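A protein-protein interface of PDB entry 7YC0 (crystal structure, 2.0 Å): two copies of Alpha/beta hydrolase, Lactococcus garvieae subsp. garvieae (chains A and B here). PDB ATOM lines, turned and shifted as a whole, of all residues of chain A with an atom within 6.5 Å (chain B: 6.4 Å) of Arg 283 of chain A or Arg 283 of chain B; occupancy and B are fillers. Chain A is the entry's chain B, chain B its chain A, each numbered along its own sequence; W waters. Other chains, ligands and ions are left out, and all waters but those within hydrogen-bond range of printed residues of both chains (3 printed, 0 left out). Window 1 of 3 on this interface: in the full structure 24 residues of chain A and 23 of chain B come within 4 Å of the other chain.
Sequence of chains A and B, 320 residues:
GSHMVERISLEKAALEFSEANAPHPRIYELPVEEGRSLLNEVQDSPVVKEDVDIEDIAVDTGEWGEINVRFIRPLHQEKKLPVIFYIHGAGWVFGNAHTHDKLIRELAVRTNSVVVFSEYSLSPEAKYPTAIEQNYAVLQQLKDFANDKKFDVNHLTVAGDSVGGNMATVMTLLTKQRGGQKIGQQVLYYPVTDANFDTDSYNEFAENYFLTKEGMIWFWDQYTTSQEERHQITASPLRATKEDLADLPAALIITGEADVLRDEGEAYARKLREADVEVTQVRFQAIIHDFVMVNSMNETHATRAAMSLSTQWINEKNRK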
ATOM      1  N   ILE A 253      -6.662  -2.942  22.083  1.00  0.00           N
ATOM      2  CA  ILE A 253      -5.549  -3.618  21.358  1.00  0.00           C
ATOM      3  C   ILE A 253      -4.623  -4.245  22.398  1.00  0.00           C
ATOM      4  O   ILE A 253      -3.998  -3.493  23.181  1.00  0.00           O
ATOM      5  CB  ILE A 253      -4.858  -2.616  20.421  1.00  0.00           C
ATOM      6  CG1 ILE A 253      -5.864  -2.060  19.402  1.00  0.00           C
ATOM      7  CG2 ILE A 253      -3.632  -3.246  19.790  1.00  0.00           C
ATOM      8  CD1 ILE A 253      -5.336  -0.935  18.543  1.00  0.00           C
ATOM      9  N   ILE A 254      -4.579  -5.570  22.410  1.00  0.00           N
ATOM     10  CA  ILE A 254      -3.774  -6.393  23.352  1.00  0.00           C
ATOM     11  C   ILE A 254      -2.548  -6.936  22.620  1.00  0.00           C
ATOM     12  O   ILE A 254      -2.698  -7.426  21.498  1.00  0.00           O
ATOM     13  CB  ILE A 254      -4.657  -7.505  23.951  1.00  0.00           C
ATOM     14  CG1 ILE A 254      -5.748  -6.914  24.855  1.00  0.00           C
ATOM     15  CG2 ILE A 254      -3.801  -8.514  24.663  1.00  0.00           C
ATOM     16  CD1 ILE A 254      -6.756  -7.924  25.351  1.00  0.00           C
ATOM     17  N   THR A 255      -1.366  -6.794  23.222  1.00  0.00           N
ATOM     18  CA  THR A 255      -0.093  -7.321  22.674  1.00  0.00           C
ATOM     19  C   THR A 255       0.589  -8.166  23.731  1.00  0.00           C
ATOM     20  O   THR A 255       0.289  -7.991  24.936  1.00  0.00           O
ATOM     21  CB  THR A 255       0.811  -6.213  22.132  1.00  0.00           C
ATOM     22  OG1 THR A 255       1.107  -5.290  23.191  1.00  0.00           O
ATOM     23  CG2 THR A 255       0.192  -5.517  20.930  1.00  0.00           C
ATOM     24  N   GLY A 256       1.438  -9.083  23.265  1.00  0.00           N
ATOM     25  CA  GLY A 256       2.337  -9.879  24.112  1.00  0.00           C
ATOM     26  C   GLY A 256       3.745  -9.382  23.914  1.00  0.00           C
ATOM     27  O   GLY A 256       4.045  -8.898  22.814  1.00  0.00           O
ATOM     28  N   GLU A 257       4.579  -9.507  24.932  1.00  0.00           N
ATOM     29  CA  GLU A 257       5.950  -8.967  24.939  1.00  0.00           C
ATOM     30  C   GLU A 257       6.772  -9.719  23.903  1.00  0.00           C
ATOM     31  O   GLU A 257       7.485  -9.042  23.154  1.00  0.00           O
ATOM     32  CB  GLU A 257       6.572  -9.065  26.328  1.00  0.00           C
ATOM     33  CG  GLU A 257       8.069  -8.805  26.344  1.00  0.00           C
ATOM     34  CD  GLU A 257       8.653  -8.959  27.737  1.00  0.00           C
ATOM     35  OE1 GLU A 257       8.102  -9.802  28.496  1.00  0.00           O
ATOM     36  OE2 GLU A 257       9.627  -8.222  28.067  1.00  0.00           O
ATOM     37  N   ARG A 262       4.382  -7.489  18.039  1.00  0.00           N
ATOM     38  CA  ARG A 262       4.141  -6.576  19.174  1.00  0.00           C
ATOM     39  C   ARG A 262       4.235  -5.131  18.694  1.00  0.00           C
ATOM     40  O   ARG A 262       3.315  -4.335  18.997  1.00  0.00           O
ATOM     41  CB  ARG A 262       5.153  -6.862  20.282  1.00  0.00           C
ATOM     42  CG  ARG A 262       5.049  -5.937  21.474  1.00  0.00           C
ATOM     43  CD  ARG A 262       6.211  -6.193  22.384  1.00  0.00           C
ATOM     44  NE  ARG A 262       7.363  -5.429  21.920  1.00  0.00           N
ATOM     45  CZ  ARG A 262       8.586  -5.535  22.401  1.00  0.00           C
ATOM     46  NH1 ARG A 262       8.884  -6.399  23.371  1.00  0.00           N
ATOM     47  NH2 ARG A 262       9.506  -4.722  21.926  1.00  0.00           N
ATOM     48  N   ASP A 263       5.311  -4.783  17.993  1.00  0.00           N
ATOM     49  CA  ASP A 263       5.557  -3.354  17.660  1.00  0.00           C
ATOM     50  C   ASP A 263       4.480  -2.838  16.698  1.00  0.00           C
ATOM     51  O   ASP A 263       3.971  -1.702  16.935  1.00  0.00           O
ATOM     52  CB  ASP A 263       6.994  -3.134  17.181  1.00  0.00           C
ATOM     53  CG  ASP A 263       8.003  -3.206  18.323  1.00  0.00           C
ATOM     54  OD1 ASP A 263       7.568  -3.306  19.538  1.00  0.00           O
ATOM     55  OD2 ASP A 263       9.215  -3.181  18.005  1.00  0.00           O
ATOM     56  N   GLU A 266       1.289  -2.169  18.643  1.00  0.00           N
ATOM     57  CA  GLU A 266       1.469  -0.950  19.478  1.00  0.00           C
ATOM     58  C   GLU A 266       1.488   0.297  18.588  1.00  0.00           C
ATOM     59  O   GLU A 266       0.874   1.312  18.994  1.00  0.00           O
ATOM     60  CB  GLU A 266       2.695  -1.134  20.371  1.00  0.00           C
ATOM     61  CG  GLU A 266       2.351  -2.043  21.538  1.00  0.00           C
ATOM     62  CD  GLU A 266       3.483  -2.578  22.387  1.00  0.00           C
ATOM     63  OE1 GLU A 266       4.621  -2.095  22.253  1.00  0.00           O
ATOM     64  OE2 GLU A 266       3.211  -3.498  23.181  1.00  0.00           O
ATOM     65  N   GLN A 281      -4.769   0.354  24.996  1.00  0.00           N
ATOM     66  CA  GLN A 281      -3.649  -0.509  24.553  1.00  0.00           C
ATOM     67  C   GLN A 281      -2.934  -1.033  25.801  1.00  0.00           C
ATOM     68  O   GLN A 281      -2.523  -0.220  26.663  1.00  0.00           O
ATOM     69  CB  GLN A 281      -2.739   0.222  23.567  1.00  0.00           C
ATOM     70  CG  GLN A 281      -1.918  -0.715  22.685  1.00  0.00           C
ATOM     71  CD  GLN A 281      -0.889  -1.546  23.401  1.00  0.00           C
ATOM     72  OE1 GLN A 281      -0.066  -1.031  24.168  1.00  0.00           O
ATOM     73  NE2 GLN A 281      -0.899  -2.841  23.124  1.00  0.00           N
ATOM     74  N   VAL A 282      -2.808  -2.356  25.879  1.00  0.00           N
ATOM     75  CA  VAL A 282      -2.216  -3.102  27.024  1.00  0.00           C
ATOM     76  C   VAL A 282      -1.268  -4.173  26.488  1.00  0.00           C
ATOM     77  O   VAL A 282      -1.667  -4.913  25.566  1.00  0.00           O
ATOM     78  CB  VAL A 282      -3.332  -3.724  27.873  1.00  0.00           C
ATOM     79  CG1 VAL A 282      -2.760  -4.697  28.873  1.00  0.00           C
ATOM     80  CG2 VAL A 282      -4.150  -2.658  28.575  1.00  0.00           C
ATOM     81  N   ARG A 283      -0.037  -4.215  26.997  1.00  0.00           N
ATOM     82  CA  ARG A 283       0.963  -5.268  26.684  1.00  0.00           C
ATOM     83  C   ARG A 283       1.141  -6.170  27.881  1.00  0.00           C
ATOM     84  O   ARG A 283       1.465  -5.638  28.971  1.00  0.00           O
ATOM     85  CB  ARG A 283       2.350  -4.703  26.383  1.00  0.00           C
ATOM     86  CG  ARG A 283       3.379  -5.746  25.993  1.00  0.00           C
ATOM     87  CD  ARG A 283       4.803  -5.258  26.267  1.00  0.00           C
ATOM     88  NE  ARG A 283       5.163  -4.244  25.283  1.00  0.00           N
ATOM     89  CZ  ARG A 283       6.392  -3.766  25.095  1.00  0.00           C
ATOM     90  NH1 ARG A 283       7.372  -4.135  25.884  1.00  0.00           N
ATOM     91  NH2 ARG A 283       6.627  -2.889  24.139  1.00  0.00           N
ATOM     92  N   PHE A 284       1.022  -7.481  27.654  1.00  0.00           N
ATOM     93  CA  PHE A 284       1.215  -8.508  28.700  1.00  0.00           C
ATOM     94  C   PHE A 284       2.641  -9.035  28.612  1.00  0.00           C
ATOM     95  O   PHE A 284       3.070  -9.434  27.521  1.00  0.00           O
ATOM     96  CB  PHE A 284       0.180  -9.622  28.540  1.00  0.00           C
ATOM     97  CG  PHE A 284      -1.218  -9.120  28.783  1.00  0.00           C
ATOM     98  CD1 PHE A 284      -1.951  -8.530  27.772  1.00  0.00           C
ATOM     99  CD2 PHE A 284      -1.758  -9.159  30.045  1.00  0.00           C
ATOM    100  CE1 PHE A 284      -3.208  -8.011  28.026  1.00  0.00           C
ATOM    101  CE2 PHE A 284      -3.030  -8.684  30.284  1.00  0.00           C
ATOM    102  CZ  PHE A 284      -3.753  -8.112  29.277  1.00  0.00           C
ATOM    103  N   GLN A 285       3.322  -9.077  29.754  1.00  0.00           N
ATOM    104  CA  GLN A 285       4.749  -9.467  29.859  1.00  0.00           C
ATOM    105  C   GLN A 285       4.878 -10.970  29.612  1.00  0.00           C
ATOM    106  O   GLN A 285       3.950 -11.704  29.968  1.00  0.00           O
ATOM    107  CB  GLN A 285       5.329  -9.102  31.237  1.00  0.00           C
ATOM    108  CG  GLN A 285       6.845  -8.911  31.205  1.00  0.00           C
ATOM    109  CD  GLN A 285       7.471  -8.660  32.560  1.00  0.00           C
ATOM    110  OE1 GLN A 285       7.158  -9.296  33.569  1.00  0.00           O
ATOM    111  NE2 GLN A 285       8.399  -7.723  32.586  1.00  0.00           N
ATOM    112  N   ILE B 253       1.562  -6.648  38.972  1.00  0.00           N
ATOM    113  CA  ILE B 253       2.483  -5.487  38.793  1.00  0.00           C
ATOM    114  C   ILE B 253       2.059  -4.722  37.540  1.00  0.00           C
ATOM    115  O   ILE B 253       2.190  -5.274  36.418  1.00  0.00           O
ATOM    116  CB  ILE B 253       3.959  -5.940  38.767  1.00  0.00           C
ATOM    117  CG1 ILE B 253       4.336  -6.580  40.103  1.00  0.00           C
ATOM    118  CG2 ILE B 253       4.870  -4.770  38.435  1.00  0.00           C
ATOM    119  CD1 ILE B 253       5.632  -7.342  40.082  1.00  0.00           C
ATOM    120  N   ILE B 254       1.601  -3.491  37.736  1.00  0.00           N
ATOM    121  CA  ILE B 254       1.056  -2.637  36.659  1.00  0.00           C
ATOM    122  C   ILE B 254       2.083  -1.558  36.365  1.00  0.00           C
ATOM    123  O   ILE B 254       2.536  -0.927  37.305  1.00  0.00           O
ATOM    124  CB  ILE B 254      -0.321  -2.083  37.052  1.00  0.00           C
ATOM    125  CG1 ILE B 254      -1.389  -3.172  36.935  1.00  0.00           C
ATOM    126  CG2 ILE B 254      -0.669  -0.844  36.243  1.00  0.00           C
ATOM    127  CD1 ILE B 254      -2.655  -2.874  37.740  1.00  0.00           C
ATOM    128  N   THR B 255       2.435  -1.371  35.098  1.00  0.00           N
ATOM    129  CA  THR B 255       3.368  -0.294  34.681  1.00  0.00           C
ATOM    130  C   THR B 255       2.689   0.556  33.622  1.00  0.00           C
ATOM    131  O   THR B 255       1.674   0.109  33.009  1.00  0.00           O
ATOM    132  CB  THR B 255       4.739  -0.816  34.201  1.00  0.00           C
ATOM    133  OG1 THR B 255       4.605  -1.773  33.147  1.00  0.00           O
ATOM    134  CG2 THR B 255       5.568  -1.408  35.323  1.00  0.00           C
ATOM    135  N   GLY B 256       3.194   1.784  33.497  1.00  0.00           N
ATOM    136  CA  GLY B 256       2.887   2.709  32.402  1.00  0.00           C
ATOM    137  C   GLY B 256       4.088   2.878  31.498  1.00  0.00           C
ATOM    138  O   GLY B 256       5.246   2.752  31.978  1.00  0.00           O
ATOM    139  N   GLU B 257       3.821   3.153  30.230  1.00  0.00           N
ATOM    140  CA  GLU B 257       4.864   3.212  29.180  1.00  0.00           C
ATOM    141  C   GLU B 257       5.820   4.382  29.439  1.00  0.00           C
ATOM    142  O   GLU B 257       7.021   4.201  29.256  1.00  0.00           O
ATOM    143  CB  GLU B 257       4.195   3.389  27.824  1.00  0.00           C
ATOM    144  CG  GLU B 257       5.184   3.466  26.684  1.00  0.00           C
ATOM    145  CD  GLU B 257       4.492   3.758  25.366  1.00  0.00           C
ATOM    146  OE1 GLU B 257       3.345   4.230  25.399  1.00  0.00           O
ATOM    147  OE2 GLU B 257       5.138   3.568  24.339  1.00  0.00           O
ATOM    148  N   ARG B 262       9.329   2.414  34.810  1.00  0.00           N
ATOM    149  CA  ARG B 262       8.742   1.312  34.019  1.00  0.00           C
ATOM    150  C   ARG B 262       9.686   0.106  34.067  1.00  0.00           C
ATOM    151  O   ARG B 262       9.242  -0.987  34.436  1.00  0.00           O
ATOM    152  CB  ARG B 262       8.495   1.780  32.582  1.00  0.00           C
ATOM    153  CG  ARG B 262       7.963   0.702  31.660  1.00  0.00           C
ATOM    154  CD  ARG B 262       7.918   1.297  30.279  1.00  0.00           C
ATOM    155  NE  ARG B 262       9.159   1.151  29.574  1.00  0.00           N
ATOM    156  CZ  ARG B 262       9.428   1.725  28.417  1.00  0.00           C
ATOM    157  NH1 ARG B 262       8.590   2.590  27.868  1.00  0.00           N
ATOM    158  NH2 ARG B 262      10.579   1.466  27.835  1.00  0.00           N
ATOM    159  N   ASP B 263      10.946   0.301  33.705  1.00  0.00           N
ATOM    160  CA  ASP B 263      11.879  -0.834  33.496  1.00  0.00           C
ATOM    161  C   ASP B 263      12.144  -1.538  34.836  1.00  0.00           C
ATOM    162  O   ASP B 263      12.226  -2.767  34.829  1.00  0.00           O
ATOM    163  CB  ASP B 263      13.149  -0.361  32.785  1.00  0.00           C
ATOM    164  CG  ASP B 263      12.953  -0.028  31.302  1.00  0.00           C
ATOM    165  OD1 ASP B 263      11.848  -0.226  30.799  1.00  0.00           O
ATOM    166  OD2 ASP B 263      13.899   0.502  30.684  1.00  0.00           O
ATOM    167  N   GLU B 266       9.128  -3.727  35.633  1.00  0.00           N
ATOM    168  CA  GLU B 266       9.071  -4.900  34.735  1.00  0.00           C
ATOM    169  C   GLU B 266      10.214  -5.855  35.066  1.00  0.00           C
ATOM    170  O   GLU B 266      10.002  -7.118  35.005  1.00  0.00           O
ATOM    171  CB  GLU B 266       9.022  -4.366  33.308  1.00  0.00           C
ATOM    172  CG  GLU B 266       7.679  -3.717  33.022  1.00  0.00           C
ATOM    173  CD  GLU B 266       7.568  -3.028  31.668  1.00  0.00           C
ATOM    174  OE1 GLU B 266       8.521  -3.139  30.901  1.00  0.00           O
ATOM    175  OE2 GLU B 266       6.533  -2.382  31.396  1.00  0.00           O
ATOM    176  N   GLN B 281       1.965  -9.361  35.014  1.00  0.00           N
ATOM    177  CA  GLN B 281       2.622  -8.064  34.698  1.00  0.00           C
ATOM    178  C   GLN B 281       1.986  -7.492  33.424  1.00  0.00           C
ATOM    179  O   GLN B 281       1.928  -8.175  32.381  1.00  0.00           O
ATOM    180  CB  GLN B 281       4.150  -8.212  34.635  1.00  0.00           C
ATOM    181  CG  GLN B 281       4.892  -6.895  34.824  1.00  0.00           C
ATOM    182  CD  GLN B 281       4.650  -5.906  33.715  1.00  0.00           C
ATOM    183  OE1 GLN B 281       4.778  -6.247  32.539  1.00  0.00           O
ATOM    184  NE2 GLN B 281       4.290  -4.673  34.075  1.00  0.00           N
ATOM    185  N   VAL B 282       1.473  -6.266  33.536  1.00  0.00           N
ATOM    186  CA  VAL B 282       0.779  -5.581  32.429  1.00  0.00           C
ATOM    187  C   VAL B 282       1.328  -4.163  32.330  1.00  0.00           C
ATOM    188  O   VAL B 282       1.441  -3.508  33.378  1.00  0.00           O
ATOM    189  CB  VAL B 282      -0.735  -5.605  32.668  1.00  0.00           C
ATOM    190  CG1 VAL B 282      -1.428  -4.971  31.504  1.00  0.00           C
ATOM    191  CG2 VAL B 282      -1.261  -7.010  32.881  1.00  0.00           C
ATOM    192  N   ARG B 283       1.639  -3.715  31.109  1.00  0.00           N
ATOM    193  CA  ARG B 283       2.055  -2.315  30.796  1.00  0.00           C
ATOM    194  C   ARG B 283       0.955  -1.635  29.979  1.00  0.00           C
ATOM    195  O   ARG B 283       0.565  -2.196  28.928  1.00  0.00           O
ATOM    196  CB  ARG B 283       3.386  -2.268  30.039  1.00  0.00           C
ATOM    197  CG  ARG B 283       3.774  -0.874  29.570  1.00  0.00           C
ATOM    198  CD  ARG B 283       4.723  -0.908  28.388  1.00  0.00           C
ATOM    199  NE  ARG B 283       6.026  -1.432  28.751  1.00  0.00           N
ATOM    200  CZ  ARG B 283       7.069  -1.418  27.922  1.00  0.00           C
ATOM    201  NH1 ARG B 283       6.969  -0.900  26.707  1.00  0.00           N
ATOM    202  NH2 ARG B 283       8.225  -1.886  28.317  1.00  0.00           N
ATOM    203  N   PHE B 284       0.496  -0.465  30.439  1.00  0.00           N
ATOM    204  CA  PHE B 284      -0.542   0.351  29.764  1.00  0.00           C
ATOM    205  C   PHE B 284       0.193   1.388  28.929  1.00  0.00           C
ATOM    206  O   PHE B 284       1.081   2.087  29.472  1.00  0.00           O
ATOM    207  CB  PHE B 284      -1.490   0.972  30.792  1.00  0.00           C
ATOM    208  CG  PHE B 284      -2.260  -0.074  31.546  1.00  0.00           C
ATOM    209  CD1 PHE B 284      -1.679  -0.772  32.594  1.00  0.00           C
ATOM    210  CD2 PHE B 284      -3.538  -0.422  31.159  1.00  0.00           C
ATOM    211  CE1 PHE B 284      -2.367  -1.784  33.241  1.00  0.00           C
ATOM    212  CE2 PHE B 284      -4.230  -1.428  31.820  1.00  0.00           C
ATOM    213  CZ  PHE B 284      -3.657  -2.090  32.873  1.00  0.00           C
ATOM    214  N   GLN B 285      -0.114   1.438  27.636  1.00  0.00           N
ATOM    215  CA  GLN B 285       0.499   2.381  26.673  1.00  0.00           C
ATOM    216  C   GLN B 285       0.119   3.819  27.032  1.00  0.00           C
ATOM    217  O   GLN B 285      -0.950   4.040  27.617  1.00  0.00           O
ATOM    218  CB  GLN B 285       0.015   2.095  25.246  1.00  0.00           C
ATOM    219  CG  GLN B 285       0.958   2.637  24.185  1.00  0.00           C
ATOM    220  CD  GLN B 285       0.491   2.339  22.777  1.00  0.00           C
ATOM    221  OE1 GLN B 285      -0.668   2.543  22.441  1.00  0.00           O
ATOM    222  NE2 GLN B 285       1.399   1.863  21.947  1.00  0.00           N
HETATM  223  O   HOH W   1       4.551  -5.871  29.751  1.00  0.00           O
HETATM  224  O   HOH W   2       1.692  -0.933  26.367  1.00  0.00           O
HETATM  225  O   HOH W   3       9.223  -1.467  24.990  1.00  0.00           O
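Water W2 lies within hydrogen-bond range of OE1 of Gln 281 of chain A (2.8 Å), O of Arg 283 of chain B (3.1 Å) and N of Gln 285 of chain B (3.2 Å). Water W1 lies within hydrogen-bond range of OE1 of Gln 281 of chain B, O of Arg 283 of chain A and N of Gln 285 of chain A. Water W3 bridges NH1 of Arg 283 of chain B (2.9 Å) and NH2 of Arg 283 of chain A (3.1 Å).
O of Arg 283 of chain B sits at hydrogen-bond distance from N of Arg 283 of chain A (2.9 Å). The side-chain amide nitrogen (NE2) of Gln 285 of chain B lies within hydrogen-bond range of the backbone carbonyl oxygen (O) of Glu 266 of chain A, 3.0 Å away. O of Glu 266 of chain B lies within hydrogen-bond range of NE2 of Gln 285 of chain A (3.0 Å). The backbone carbonyl oxygen (O) of Gln 281 of chain B sits at hydrogen-bond distance from the backbone NH (N) of Gln 285 of chain A. The backbone carbonyl oxygen (O) of Gln 281 of chain A is in hydrogen-bond range of the backbone NH (N) of Gln 285 of chain B.
Gln 281 of chain A touches Phe 284 of chain B (O to CA, 3.7 Å). Val 282 of chain A touches Val 282 of chain B (CG1 to CG1, 3.0 Å). Arg 283 of chain B touches Val 282 of chain A. Phe 284 of chain B touches Val 282 of chain A. Arg 283 of chain A touches Val 282 of chain B. Phe 284 of chain A touches Gln 281 of chain B (CA to O, 3.8 Å). CE2 of Phe 284 of chain A touches CG2 of Val 282 of chain B, at 3.6 Å.
Glu 266 of chain A touches Gln 285 of chain B, and with the chains exchanged Gln 285 of chain A touches Glu 266 of chain B. Gln 281 of chain A touches Phe 284 of chain B, and with the chains exchanged Phe 284 of chain A touches Gln 281 of chain B. Val 282 of chain B touches its own counterpart, Val 282 of chain A. Val 282 of chain A touches Arg 283 of chain B, and with the chains exchanged Arg 283 of chain A touches Val 282 of chain B. Positions printed for both chains: 253, 254, 255, 256, 257, 262, 263, 266, 281, 282, 283, 284 and 285. Of the 12 pairs that touch across the chains among the printed residues, 12 have their exchanged pair printed and touching as well.
Hydrophobic or aromatic side chains of chain B that line the printed part of chain A: Val 282 and Phe 284. Among the printed residues, no Asp or Glu carboxylate lies within 4 Å of a Lys or Arg side-chain nitrogen of the other chain.
NH2 of Arg 283 of chain A is in salt-bridge range of OE1 of Glu 266 of chain A, 2.9 Å away. NE2 of Gln 281 of chain A is in hydrogen-bond range of OG1 of Thr 255 of chain A, at 3.2 Å. The backbone NH (N) of Val 282 of chain B lies within hydrogen-bond range of the backbone carbonyl oxygen (O) of Ile 253 of chain B (3.1 Å). The backbone NH (N) of Thr 255 of chain B is in hydrogen-bond range of the backbone carbonyl oxygen (O) of Val 282 of chain B. O of Thr 255 of chain B lies within hydrogen-bond range of N of Phe 284 of chain B, 2.9 Å away. OE2 of Glu 266 of chain B sits at hydrogen-bond distance from OG1 of Thr 255 of chain B.
Of the printed residues of chain B, Gln 281 of chain A touches Phe 284 (3.7 Å) and Gln 285 (3.1 Å). Of chain B, only Val 282 and Arg 283 come within 4 Å of Arg 283 of chain A. Of the printed residues of chain A, Glu 266 of chain B touches Gln 285. Of the printed residues of chain A, Val 282 of chain B touches Val 282, Arg 283 and Phe 284. Of chain A, only Val 282 and Arg 283 come within 4 Å of Arg 283 of chain B. The nearest residue of chain B that does not touch Arg 283 of chain A is Gln 281 of chain B (4.3 Å).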
